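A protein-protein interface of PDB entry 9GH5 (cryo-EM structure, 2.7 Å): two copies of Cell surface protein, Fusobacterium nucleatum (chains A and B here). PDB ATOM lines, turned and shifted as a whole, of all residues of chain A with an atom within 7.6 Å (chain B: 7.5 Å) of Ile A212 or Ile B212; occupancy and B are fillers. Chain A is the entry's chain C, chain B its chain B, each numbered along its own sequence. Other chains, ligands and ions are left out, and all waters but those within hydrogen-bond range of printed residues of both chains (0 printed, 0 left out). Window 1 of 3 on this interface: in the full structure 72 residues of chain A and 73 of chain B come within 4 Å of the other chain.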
ATOM      1  N   VAL A 201      10.920  17.527  38.587  1.00  0.00           N
ATOM      2  CA  VAL A 201       9.463  17.509  38.540  1.00  0.00           C
ATOM      3  C   VAL A 201       9.044  16.116  38.098  1.00  0.00           C
ATOM      4  O   VAL A 201       9.438  15.657  37.020  1.00  0.00           O
ATOM      5  CB  VAL A 201       8.904  18.579  37.592  1.00  0.00           C
ATOM      6  CG1 VAL A 201       7.465  18.265  37.230  1.00  0.00           C
ATOM      7  CG2 VAL A 201       9.001  19.944  38.237  1.00  0.00           C
ATOM      8  N   VAL A 203       6.089  13.296  37.220  1.00  0.00           N
ATOM      9  CA  VAL A 203       4.723  13.113  36.756  1.00  0.00           C
ATOM     10  C   VAL A 203       4.289  11.654  36.870  1.00  0.00           C
ATOM     11  O   VAL A 203       3.407  11.211  36.149  1.00  0.00           O
ATOM     12  CB  VAL A 203       4.552  13.632  35.315  1.00  0.00           C
ATOM     13  CG1 VAL A 203       4.542  15.149  35.298  1.00  0.00           C
ATOM     14  CG2 VAL A 203       5.657  13.093  34.425  1.00  0.00           C
ATOM     15  N   LYS A 209       3.789   5.684  34.537  1.00  0.00           N
ATOM     16  CA  LYS A 209       4.429   6.845  33.937  1.00  0.00           C
ATOM     17  C   LYS A 209       3.419   7.558  33.052  1.00  0.00           C
ATOM     18  O   LYS A 209       2.779   6.929  32.204  1.00  0.00           O
ATOM     19  CB  LYS A 209       5.658   6.430  33.129  1.00  0.00           C
ATOM     20  CG  LYS A 209       6.723   5.747  33.966  1.00  0.00           C
ATOM     21  CD  LYS A 209       7.904   5.313  33.124  1.00  0.00           C
ATOM     22  CE  LYS A 209       9.142   5.144  33.983  1.00  0.00           C
ATOM     23  NZ  LYS A 209       9.224   3.779  34.569  1.00  0.00           N
ATOM     24  N   ARG A 210       3.282   8.863  33.249  1.00  0.00           N
ATOM     25  CA  ARG A 210       2.292   9.658  32.540  1.00  0.00           C
ATOM     26  C   ARG A 210       2.899  10.301  31.302  1.00  0.00           C
ATOM     27  O   ARG A 210       4.075  10.670  31.282  1.00  0.00           O
ATOM     28  CB  ARG A 210       1.716  10.746  33.447  1.00  0.00           C
ATOM     29  CG  ARG A 210       0.706  10.251  34.461  1.00  0.00           C
ATOM     30  CD  ARG A 210       0.242  11.386  35.355  1.00  0.00           C
ATOM     31  NE  ARG A 210      -0.769  10.950  36.309  1.00  0.00           N
ATOM     32  CZ  ARG A 210      -0.499  10.403  37.485  1.00  0.00           C
ATOM     33  NH1 ARG A 210       0.746  10.224  37.893  1.00  0.00           N
ATOM     34  NH2 ARG A 210      -1.502  10.027  38.271  1.00  0.00           N
ATOM     35  N   LYS A 211       2.080  10.429  30.266  1.00  0.00           N
ATOM     36  CA  LYS A 211       2.449  11.182  29.079  1.00  0.00           C
ATOM     37  C   LYS A 211       2.113  12.653  29.282  1.00  0.00           C
ATOM     38  O   LYS A 211       1.197  13.003  30.030  1.00  0.00           O
ATOM     39  CB  LYS A 211       1.717  10.654  27.846  1.00  0.00           C
ATOM     40  CG  LYS A 211       2.170   9.288  27.378  1.00  0.00           C
ATOM     41  CD  LYS A 211       1.224   8.741  26.325  1.00  0.00           C
ATOM     42  CE  LYS A 211       1.171   9.651  25.111  1.00  0.00           C
ATOM     43  NZ  LYS A 211       0.347   9.070  24.017  1.00  0.00           N
ATOM     44  N   ILE A 212       2.864  13.515  28.605  1.00  0.00           N
ATOM     45  CA  ILE A 212       2.599  14.947  28.604  1.00  0.00           C
ATOM     46  C   ILE A 212       2.091  15.304  27.214  1.00  0.00           C
ATOM     47  O   ILE A 212       2.851  15.275  26.238  1.00  0.00           O
ATOM     48  CB  ILE A 212       3.841  15.763  28.979  1.00  0.00           C
ATOM     49  CG1 ILE A 212       4.453  15.226  30.272  1.00  0.00           C
ATOM     50  CG2 ILE A 212       3.475  17.223  29.159  1.00  0.00           C
ATOM     51  CD1 ILE A 212       5.782  15.848  30.619  1.00  0.00           C
ATOM     52  N   VAL A 213       0.812  15.640  27.124  1.00  0.00           N
ATOM     53  CA  VAL A 213       0.157  15.862  25.854  1.00  0.00           C
ATOM     54  C   VAL A 213      -0.035  17.360  25.640  1.00  0.00           C
ATOM     55  O   VAL A 213       0.094  18.164  26.561  1.00  0.00           O
ATOM     56  CB  VAL A 213      -1.193  15.113  25.768  1.00  0.00           C
ATOM     57  CG1 VAL A 213      -0.968  13.631  25.529  1.00  0.00           C
ATOM     58  CG2 VAL A 213      -1.997  15.330  27.035  1.00  0.00           C
ATOM     59  N   ASN A 214      -0.350  17.739  24.401  1.00  0.00           N
ATOM     60  CA  ASN A 214      -0.651  19.125  24.040  1.00  0.00           C
ATOM     61  C   ASN A 214       0.508  20.056  24.389  1.00  0.00           C
ATOM     62  O   ASN A 214       0.325  21.126  24.973  1.00  0.00           O
ATOM     63  CB  ASN A 214      -1.950  19.589  24.701  1.00  0.00           C
ATOM     64  CG  ASN A 214      -3.157  18.819  24.211  1.00  0.00           C
ATOM     65  OD1 ASN A 214      -3.143  18.251  23.122  1.00  0.00           O
ATOM     66  ND2 ASN A 214      -4.207  18.790  25.021  1.00  0.00           N
ATOM     67  N   VAL A 215       1.713  19.639  24.023  1.00  0.00           N
ATOM     68  CA  VAL A 215       2.915  20.428  24.260  1.00  0.00           C
ATOM     69  C   VAL A 215       3.243  21.210  22.998  1.00  0.00           C
ATOM     70  O   VAL A 215       3.260  20.649  21.896  1.00  0.00           O
ATOM     71  CB  VAL A 215       4.094  19.530  24.670  1.00  0.00           C
ATOM     72  CG1 VAL A 215       5.295  20.375  25.052  1.00  0.00           C
ATOM     73  CG2 VAL A 215       3.692  18.626  25.816  1.00  0.00           C
ATOM     74  N   GLY A 216       3.494  22.505  23.154  1.00  0.00           N
ATOM     75  CA  GLY A 216       3.903  23.311  22.027  1.00  0.00           C
ATOM     76  C   GLY A 216       5.282  22.932  21.528  1.00  0.00           C
ATOM     77  O   GLY A 216       6.085  22.315  22.229  1.00  0.00           O
ATOM     78  N   ASP A 217       5.554  23.305  20.280  1.00  0.00           N
ATOM     79  CA  ASP A 217       6.831  22.968  19.666  1.00  0.00           C
ATOM     80  C   ASP A 217       7.979  23.618  20.425  1.00  0.00           C
ATOM     81  O   ASP A 217       7.867  24.747  20.908  1.00  0.00           O
ATOM     82  CB  ASP A 217       6.851  23.412  18.204  1.00  0.00           C
ATOM     83  CG  ASP A 217       6.096  22.464  17.300  1.00  0.00           C
ATOM     84  OD1 ASP A 217       5.230  21.722  17.809  1.00  0.00           O
ATOM     85  OD2 ASP A 217       6.369  22.458  16.081  1.00  0.00           O
ATOM     86  N   GLY A 218       9.088  22.894  20.527  1.00  0.00           N
ATOM     87  CA  GLY A 218      10.256  23.404  21.215  1.00  0.00           C
ATOM     88  C   GLY A 218      10.978  24.476  20.429  1.00  0.00           C
ATOM     89  O   GLY A 218      10.414  25.075  19.508  1.00  0.00           O
ATOM     90  N   ALA A 219      12.233  24.724  20.783  1.00  0.00           N
ATOM     91  CA  ALA A 219      13.037  25.795  20.206  1.00  0.00           C
ATOM     92  C   ALA A 219      14.418  25.279  19.839  1.00  0.00           C
ATOM     93  O   ALA A 219      15.438  25.851  20.227  1.00  0.00           O
ATOM     94  CB  ALA A 219      13.141  26.979  21.162  1.00  0.00           C
ATOM     95  N   SER A 225      16.444  25.557  26.309  1.00  0.00           N
ATOM     96  CA  SER A 225      15.995  24.581  27.297  1.00  0.00           C
ATOM     97  C   SER A 225      14.477  24.513  27.185  1.00  0.00           C
ATOM     98  O   SER A 225      13.754  25.204  27.905  1.00  0.00           O
ATOM     99  CB  SER A 225      16.439  24.964  28.697  1.00  0.00           C
ATOM    100  OG  SER A 225      15.681  26.057  29.183  1.00  0.00           O
ATOM    101  N   ASP A 226      14.001  23.667  26.276  1.00  0.00           N
ATOM    102  CA  ASP A 226      12.575  23.500  26.041  1.00  0.00           C
ATOM    103  C   ASP A 226      12.217  22.024  26.121  1.00  0.00           C
ATOM    104  O   ASP A 226      13.019  21.214  26.589  1.00  0.00           O
ATOM    105  CB  ASP A 226      12.181  24.081  24.684  1.00  0.00           C
ATOM    106  CG  ASP A 226      11.559  25.455  24.800  1.00  0.00           C
ATOM    107  OD1 ASP A 226      10.611  25.607  25.595  1.00  0.00           O
ATOM    108  OD2 ASP A 226      12.018  26.383  24.104  1.00  0.00           O
ATOM    109  N   ALA A 227      11.013  21.665  25.690  1.00  0.00           N
ATOM    110  CA  ALA A 227      10.593  20.270  25.622  1.00  0.00           C
ATOM    111  C   ALA A 227      10.221  19.964  24.179  1.00  0.00           C
ATOM    112  O   ALA A 227       9.219  20.478  23.671  1.00  0.00           O
ATOM    113  CB  ALA A 227       9.423  20.000  26.565  1.00  0.00           C
ATOM    114  N   VAL A 228      11.027  19.132  23.517  1.00  0.00           N
ATOM    115  CA  VAL A 228      10.711  18.768  22.143  1.00  0.00           C
ATOM    116  C   VAL A 228       9.479  17.870  22.125  1.00  0.00           C
ATOM    117  O   VAL A 228       9.132  17.212  23.113  1.00  0.00           O
ATOM    118  CB  VAL A 228      11.908  18.089  21.456  1.00  0.00           C
ATOM    119  CG1 VAL A 228      13.214  18.589  22.050  1.00  0.00           C
ATOM    120  CG2 VAL A 228      11.808  16.578  21.554  1.00  0.00           C
ATOM    121  N   THR A 229       8.799  17.858  20.987  1.00  0.00           N
ATOM    122  CA  THR A 229       7.556  17.121  20.841  1.00  0.00           C
ATOM    123  C   THR A 229       7.752  15.949  19.888  1.00  0.00           C
ATOM    124  O   THR A 229       8.835  15.731  19.338  1.00  0.00           O
ATOM    125  CB  THR A 229       6.437  18.042  20.355  1.00  0.00           C
ATOM    126  OG1 THR A 229       6.877  18.763  19.200  1.00  0.00           O
ATOM    127  CG2 THR A 229       6.063  19.033  21.442  1.00  0.00           C
ATOM    128  N   GLY A 230       6.676  15.183  19.699  1.00  0.00           N
ATOM    129  CA  GLY A 230       6.749  14.031  18.820  1.00  0.00           C
ATOM    130  C   GLY A 230       7.034  14.411  17.380  1.00  0.00           C
ATOM    131  O   GLY A 230       7.830  13.760  16.703  1.00  0.00           O
ATOM    132  N   LEU B 189      -3.266  21.296  33.461  1.00  0.00           N
ATOM    133  CA  LEU B 189      -2.585  22.515  33.868  1.00  0.00           C
ATOM    134  C   LEU B 189      -2.909  23.646  32.903  1.00  0.00           C
ATOM    135  O   LEU B 189      -2.863  23.466  31.682  1.00  0.00           O
ATOM    136  CB  LEU B 189      -1.070  22.308  33.922  1.00  0.00           C
ATOM    137  CG  LEU B 189      -0.555  21.220  34.865  1.00  0.00           C
ATOM    138  CD1 LEU B 189       0.940  21.030  34.684  1.00  0.00           C
ATOM    139  CD2 LEU B 189      -0.880  21.562  36.306  1.00  0.00           C
ATOM    140  N   ASN B 199      -4.136   8.593  32.593  1.00  0.00           N
ATOM    141  CA  ASN B 199      -2.693   8.510  32.830  1.00  0.00           C
ATOM    142  C   ASN B 199      -1.919   9.482  31.942  1.00  0.00           C
ATOM    143  O   ASN B 199      -0.894   9.132  31.353  1.00  0.00           O
ATOM    144  CB  ASN B 199      -2.184   7.080  32.644  1.00  0.00           C
ATOM    145  CG  ASN B 199      -3.146   6.046  33.189  1.00  0.00           C
ATOM    146  OD1 ASN B 199      -3.459   6.040  34.378  1.00  0.00           O
ATOM    147  ND2 ASN B 199      -3.619   5.163  32.319  1.00  0.00           N
ATOM    148  N   THR B 200      -2.413  10.714  31.840  1.00  0.00           N
ATOM    149  CA  THR B 200      -1.763  11.740  31.039  1.00  0.00           C
ATOM    150  C   THR B 200      -1.732  13.049  31.813  1.00  0.00           C
ATOM    151  O   THR B 200      -2.534  13.279  32.722  1.00  0.00           O
ATOM    152  CB  THR B 200      -2.473  11.961  29.695  1.00  0.00           C
ATOM    153  OG1 THR B 200      -3.849  12.282  29.925  1.00  0.00           O
ATOM    154  CG2 THR B 200      -2.380  10.719  28.822  1.00  0.00           C
ATOM    155  N   VAL B 201      -0.787  13.905  31.442  1.00  0.00           N
ATOM    156  CA  VAL B 201      -0.699  15.269  31.951  1.00  0.00           C
ATOM    157  C   VAL B 201      -0.848  16.201  30.759  1.00  0.00           C
ATOM    158  O   VAL B 201      -0.072  16.119  29.800  1.00  0.00           O
ATOM    159  CB  VAL B 201       0.624  15.525  32.688  1.00  0.00           C
ATOM    160  CG1 VAL B 201       0.871  17.017  32.829  1.00  0.00           C
ATOM    161  CG2 VAL B 201       0.610  14.853  34.045  1.00  0.00           C
ATOM    162  N   SER B 202      -1.841  17.081  30.813  1.00  0.00           N
ATOM    163  CA  SER B 202      -2.164  17.954  29.693  1.00  0.00           C
ATOM    164  C   SER B 202      -1.816  19.394  30.040  1.00  0.00           C
ATOM    165  O   SER B 202      -2.173  19.883  31.117  1.00  0.00           O
ATOM    166  CB  SER B 202      -3.643  17.841  29.326  1.00  0.00           C
ATOM    167  OG  SER B 202      -3.970  18.718  28.264  1.00  0.00           O
ATOM    168  N   VAL B 203      -1.123  20.067  29.126  1.00  0.00           N
ATOM    169  CA  VAL B 203      -0.742  21.460  29.296  1.00  0.00           C
ATOM    170  C   VAL B 203      -1.397  22.348  28.240  1.00  0.00           C
ATOM    171  O   VAL B 203      -0.872  23.399  27.903  1.00  0.00           O
ATOM    172  CB  VAL B 203       0.790  21.621  29.284  1.00  0.00           C
ATOM    173  CG1 VAL B 203       1.389  21.057  30.559  1.00  0.00           C
ATOM    174  CG2 VAL B 203       1.384  20.937  28.068  1.00  0.00           C
ATOM    175  N   LYS B 209      -1.613  25.195  22.480  1.00  0.00           N
ATOM    176  CA  LYS B 209      -0.616  24.270  22.995  1.00  0.00           C
ATOM    177  C   LYS B 209       0.502  25.066  23.648  1.00  0.00           C
ATOM    178  O   LYS B 209       1.057  25.983  23.034  1.00  0.00           O
ATOM    179  CB  LYS B 209      -0.066  23.384  21.878  1.00  0.00           C
ATOM    180  CG  LYS B 209      -1.126  22.532  21.210  1.00  0.00           C
ATOM    181  CD  LYS B 209      -0.549  21.707  20.077  1.00  0.00           C
ATOM    182  CE  LYS B 209      -1.417  20.495  19.797  1.00  0.00           C
ATOM    183  NZ  LYS B 209      -2.507  20.808  18.836  1.00  0.00           N
ATOM    184  N   ARG B 210       0.832  24.715  24.885  1.00  0.00           N
ATOM    185  CA  ARG B 210       1.825  25.447  25.653  1.00  0.00           C
ATOM    186  C   ARG B 210       3.204  24.822  25.491  1.00  0.00           C
ATOM    187  O   ARG B 210       3.342  23.613  25.290  1.00  0.00           O
ATOM    188  CB  ARG B 210       1.451  25.476  27.134  1.00  0.00           C
ATOM    189  CG  ARG B 210       0.360  26.467  27.484  1.00  0.00           C
ATOM    190  CD  ARG B 210       0.021  26.396  28.960  1.00  0.00           C
ATOM    191  NE  ARG B 210      -1.004  27.360  29.329  1.00  0.00           N
ATOM    192  CZ  ARG B 210      -2.307  27.151  29.199  1.00  0.00           C
ATOM    193  NH1 ARG B 210      -2.779  26.011  28.723  1.00  0.00           N
ATOM    194  NH2 ARG B 210      -3.157  28.110  29.553  1.00  0.00           N
ATOM    195  N   LYS B 211       4.225  25.664  25.582  1.00  0.00           N
ATOM    196  CA  LYS B 211       5.601  25.202  25.632  1.00  0.00           C
ATOM    197  C   LYS B 211       6.014  24.975  27.078  1.00  0.00           C
ATOM    198  O   LYS B 211       5.507  25.623  27.997  1.00  0.00           O
ATOM    199  CB  LYS B 211       6.545  26.215  24.983  1.00  0.00           C
ATOM    200  CG  LYS B 211       6.403  26.337  23.480  1.00  0.00           C
ATOM    201  CD  LYS B 211       7.175  27.537  22.963  1.00  0.00           C
ATOM    202  CE  LYS B 211       8.653  27.416  23.286  1.00  0.00           C
ATOM    203  NZ  LYS B 211       9.445  28.523  22.685  1.00  0.00           N
ATOM    204  N   ILE B 212       6.941  24.045  27.275  1.00  0.00           N
ATOM    205  CA  ILE B 212       7.520  23.780  28.585  1.00  0.00           C
ATOM    206  C   ILE B 212       8.948  24.301  28.551  1.00  0.00           C
ATOM    207  O   ILE B 212       9.815  23.726  27.882  1.00  0.00           O
ATOM    208  CB  ILE B 212       7.469  22.291  28.945  1.00  0.00           C
ATOM    209  CG1 ILE B 212       6.052  21.750  28.750  1.00  0.00           C
ATOM    210  CG2 ILE B 212       7.902  22.081  30.379  1.00  0.00           C
ATOM    211  CD1 ILE B 212       5.949  20.252  28.893  1.00  0.00           C
ATOM    212  N   VAL B 213       9.196  25.387  29.272  1.00  0.00           N
ATOM    213  CA  VAL B 213      10.468  26.072  29.225  1.00  0.00           C
ATOM    214  C   VAL B 213      11.259  25.755  30.488  1.00  0.00           C
ATOM    215  O   VAL B 213      10.727  25.245  31.471  1.00  0.00           O
ATOM    216  CB  VAL B 213      10.288  27.599  29.052  1.00  0.00           C
ATOM    217  CG1 VAL B 213       9.914  27.935  27.621  1.00  0.00           C
ATOM    218  CG2 VAL B 213       9.235  28.117  30.013  1.00  0.00           C
ATOM    219  N   ASN B 214      12.558  26.061  30.459  1.00  0.00           N
ATOM    220  CA  ASN B 214      13.442  25.895  31.611  1.00  0.00           C
ATOM    221  C   ASN B 214      13.453  24.451  32.107  1.00  0.00           C
ATOM    222  O   ASN B 214      13.304  24.181  33.299  1.00  0.00           O
ATOM    223  CB  ASN B 214      13.061  26.855  32.739  1.00  0.00           C
ATOM    224  CG  ASN B 214      13.253  28.305  32.354  1.00  0.00           C
ATOM    225  OD1 ASN B 214      14.044  28.623  31.467  1.00  0.00           O
ATOM    226  ND2 ASN B 214      12.523  29.195  33.014  1.00  0.00           N
ATOM    227  N   VAL B 215      13.626  23.516  31.181  1.00  0.00           N
ATOM    228  CA  VAL B 215      13.700  22.098  31.510  1.00  0.00           C
ATOM    229  C   VAL B 215      15.163  21.690  31.576  1.00  0.00           C
ATOM    230  O   VAL B 215      15.952  22.021  30.682  1.00  0.00           O
ATOM    231  CB  VAL B 215      12.940  21.252  30.476  1.00  0.00           C
ATOM    232  CG1 VAL B 215      12.897  19.799  30.912  1.00  0.00           C
ATOM    233  CG2 VAL B 215      11.539  21.792  30.282  1.00  0.00           C
ATOM    234  N   ASP B 226      12.831  10.440  30.879  1.00  0.00           N
ATOM    235  CA  ASP B 226      13.017  11.850  31.187  1.00  0.00           C
ATOM    236  C   ASP B 226      12.378  12.698  30.100  1.00  0.00           C
ATOM    237  O   ASP B 226      11.625  12.183  29.272  1.00  0.00           O
ATOM    238  CB  ASP B 226      14.503  12.178  31.329  1.00  0.00           C
ATOM    239  CG  ASP B 226      14.941  12.271  32.774  1.00  0.00           C
ATOM    240  OD1 ASP B 226      14.293  13.012  33.538  1.00  0.00           O
ATOM    241  OD2 ASP B 226      15.925  11.601  33.148  1.00  0.00           O
ATOM    242  N   ALA B 227      12.654  13.996  30.098  1.00  0.00           N
ATOM    243  CA  ALA B 227      12.177  14.895  29.053  1.00  0.00           C
ATOM    244  C   ALA B 227      13.391  15.537  28.398  1.00  0.00           C
ATOM    245  O   ALA B 227      14.100  16.323  29.034  1.00  0.00           O
ATOM    246  CB  ALA B 227      11.231  15.949  29.621  1.00  0.00           C
ATOM    247  N   VAL B 228      13.633  15.199  27.129  1.00  0.00           N
ATOM    248  CA  VAL B 228      14.759  15.795  26.429  1.00  0.00           C
ATOM    249  C   VAL B 228      14.463  17.264  26.146  1.00  0.00           C
ATOM    250  O   VAL B 228      13.311  17.711  26.142  1.00  0.00           O
ATOM    251  CB  VAL B 228      15.072  15.033  25.131  1.00  0.00           C
ATOM    252  CG1 VAL B 228      15.027  13.537  25.374  1.00  0.00           C
ATOM    253  CG2 VAL B 228      14.114  15.435  24.035  1.00  0.00           C
ATOM    254  N   THR B 229      15.522  18.025  25.911  1.00  0.00           N
ATOM    255  CA  THR B 229      15.402  19.454  25.672  1.00  0.00           C
ATOM    256  C   THR B 229      15.818  19.781  24.243  1.00  0.00           C
ATOM    257  O   THR B 229      16.231  18.909  23.472  1.00  0.00           O
ATOM    258  CB  THR B 229      16.235  20.244  26.681  1.00  0.00           C
ATOM    259  OG1 THR B 229      17.576  19.747  26.691  1.00  0.00           O
ATOM    260  CG2 THR B 229      15.648  20.104  28.073  1.00  0.00           C
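Of the 17 printed residues of chain B, 14 touch a printed residue of chain A.
Hydrophobic or aromatic side chains of chain B within 4 Å of the printed part of chain A: Val B201, Val B203, Ile B212, Val B213, Val B215 and Val B228.
Among the printed residues, Asp or Glu carboxylates within 4 Å of a Lys or Arg side-chain nitrogen of the other chain: Asp A226 with Lys B211 (3.6 Å).
Arg A210 touches Val B201, but with the chains exchanged Val A201 does not touch Arg B210 (13.7 Å).
Val A215 touches Val B203, but with the chains exchanged Val A203 does not touch Val B215 (10.5 Å).
Val A215 touches Ile B212, but with the chains exchanged Ile A212 does not touch Val B215 (8.1 Å).
Asp A226 touches Ile B212, but with the chains exchanged Ile A212 does not touch Asp B226 (7.0 Å).
Of the 33 pairs that touch across the chains among the printed residues, 2 have their exchanged pair printed and touching as well.
O of Val B203 lies close to NH1 of Arg B210, 3.3 Å away.
O of Val A203 sits close to NH1 of Arg A210 (3.3 Å).
The backbone NH (N) of Leu B189 is in hydrogen-bond range of the backbone carbonyl oxygen (O) of Ser B202, at 2.9 Å.
Among the printed residues, pairs that only touch across the chains: Asp A226 with Thr B229 (3.1 Å), Ile A212 with Val B201 (3.2 Å), Asp A226 with Val B213 (3.2 Å), Asn A214 with Val B203 (3.3 Å), Val A215 with Arg B210 (3.3 Å), Val A228 with Thr B229 (3.4 Å), Asp A217 with Lys B211 (3.4 Å), Lys A211 with Thr B200 (3.4 Å), Arg A210 with Asn B199 (3.4 Å), Asp A226 with Val B228 (3.5 Å), Val A228 with Val B228 (3.6 Å), Ser A225 with Val B215 (3.6 Å), Asn A214 with Arg B210 (3.6 Å), Ser A225 with Val B213 (3.6 Å), Arg A210 with Val B201 (3.7 Å), Val A213 with Ser B202 (3.7 Å), Ala A227 with Val B228 (3.8 Å), Asn A214 with Lys B209 (3.8 Å), Gly A216 with Lys B209 (3.9 Å), Asp A226 with Val B215 (3.9 Å), Val A215 with Ile B212 (3.9 Å), Ile A212 with Ile B212 (3.9 Å) and Val A215 with Val B203 (3.97 Å).
Printed residues of chain B within 4 Å of Ile A212: Val B201 (3.2 Å) and Ile B212 (3.9 Å).
Ile B212 touches just these residues of chain A: Ile A212, Val A215, Asp A226 and Ala A227.
Printed residues of chain B within 4 Å of Ala A227: Ile B212 (3.2 Å) and Val B228 (3.8 Å).
Printed residues of chain A within 4 Å of Val B215: Ser A225 (3.6 Å) and Asp A226 (3.9 Å).
Of the printed residues of chain B, Val A215 touches Val B203 (3.97 Å), Arg B210 (3.3 Å) and Ile B212 (3.9 Å).
Of the printed residues of chain A, Arg B210 touches Asn A214, Val A215 and Gly A216.
The nearest residue of chain B that does not touch Ile A212 is Val B203 (4.4 Å).
OG of Ser B202 is in hydrogen-bond range of ND2 of Asn A214 (3.3 Å).
The backbone NH (N) of Val B201 sits at hydrogen-bond distance from the backbone carbonyl oxygen (O) of Lys A211, 2.6 Å away.
The side-chain carboxylate (OD1) of Asp A226 sits close to the backbone carbonyl oxygen (O) of Ile B212.
O of Arg B210 is in hydrogen-bond range of N of Gly A216, at 2.4 Å.
The backbone carbonyl oxygen (O) of Asn B199 lies within hydrogen-bond range of the backbone NH (N) of Lys A211.
O of Val A213 sits close to N of Val B203, 3.4 Å away.
N of Val A213 lies within hydrogen-bond range of O of Val B201 (2.9 Å).
The side-chain amino group (NZ) of Lys B211 is in salt-bridge range of the side-chain carboxylate (OD2) of Asp A226, at 3.6 Å.
O of Ile B212 is in hydrogen-bond range of N of Ala A227 (3.2 Å).
N of Asn B214 is in hydrogen-bond range of O of Ser A225 (2.9 Å).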
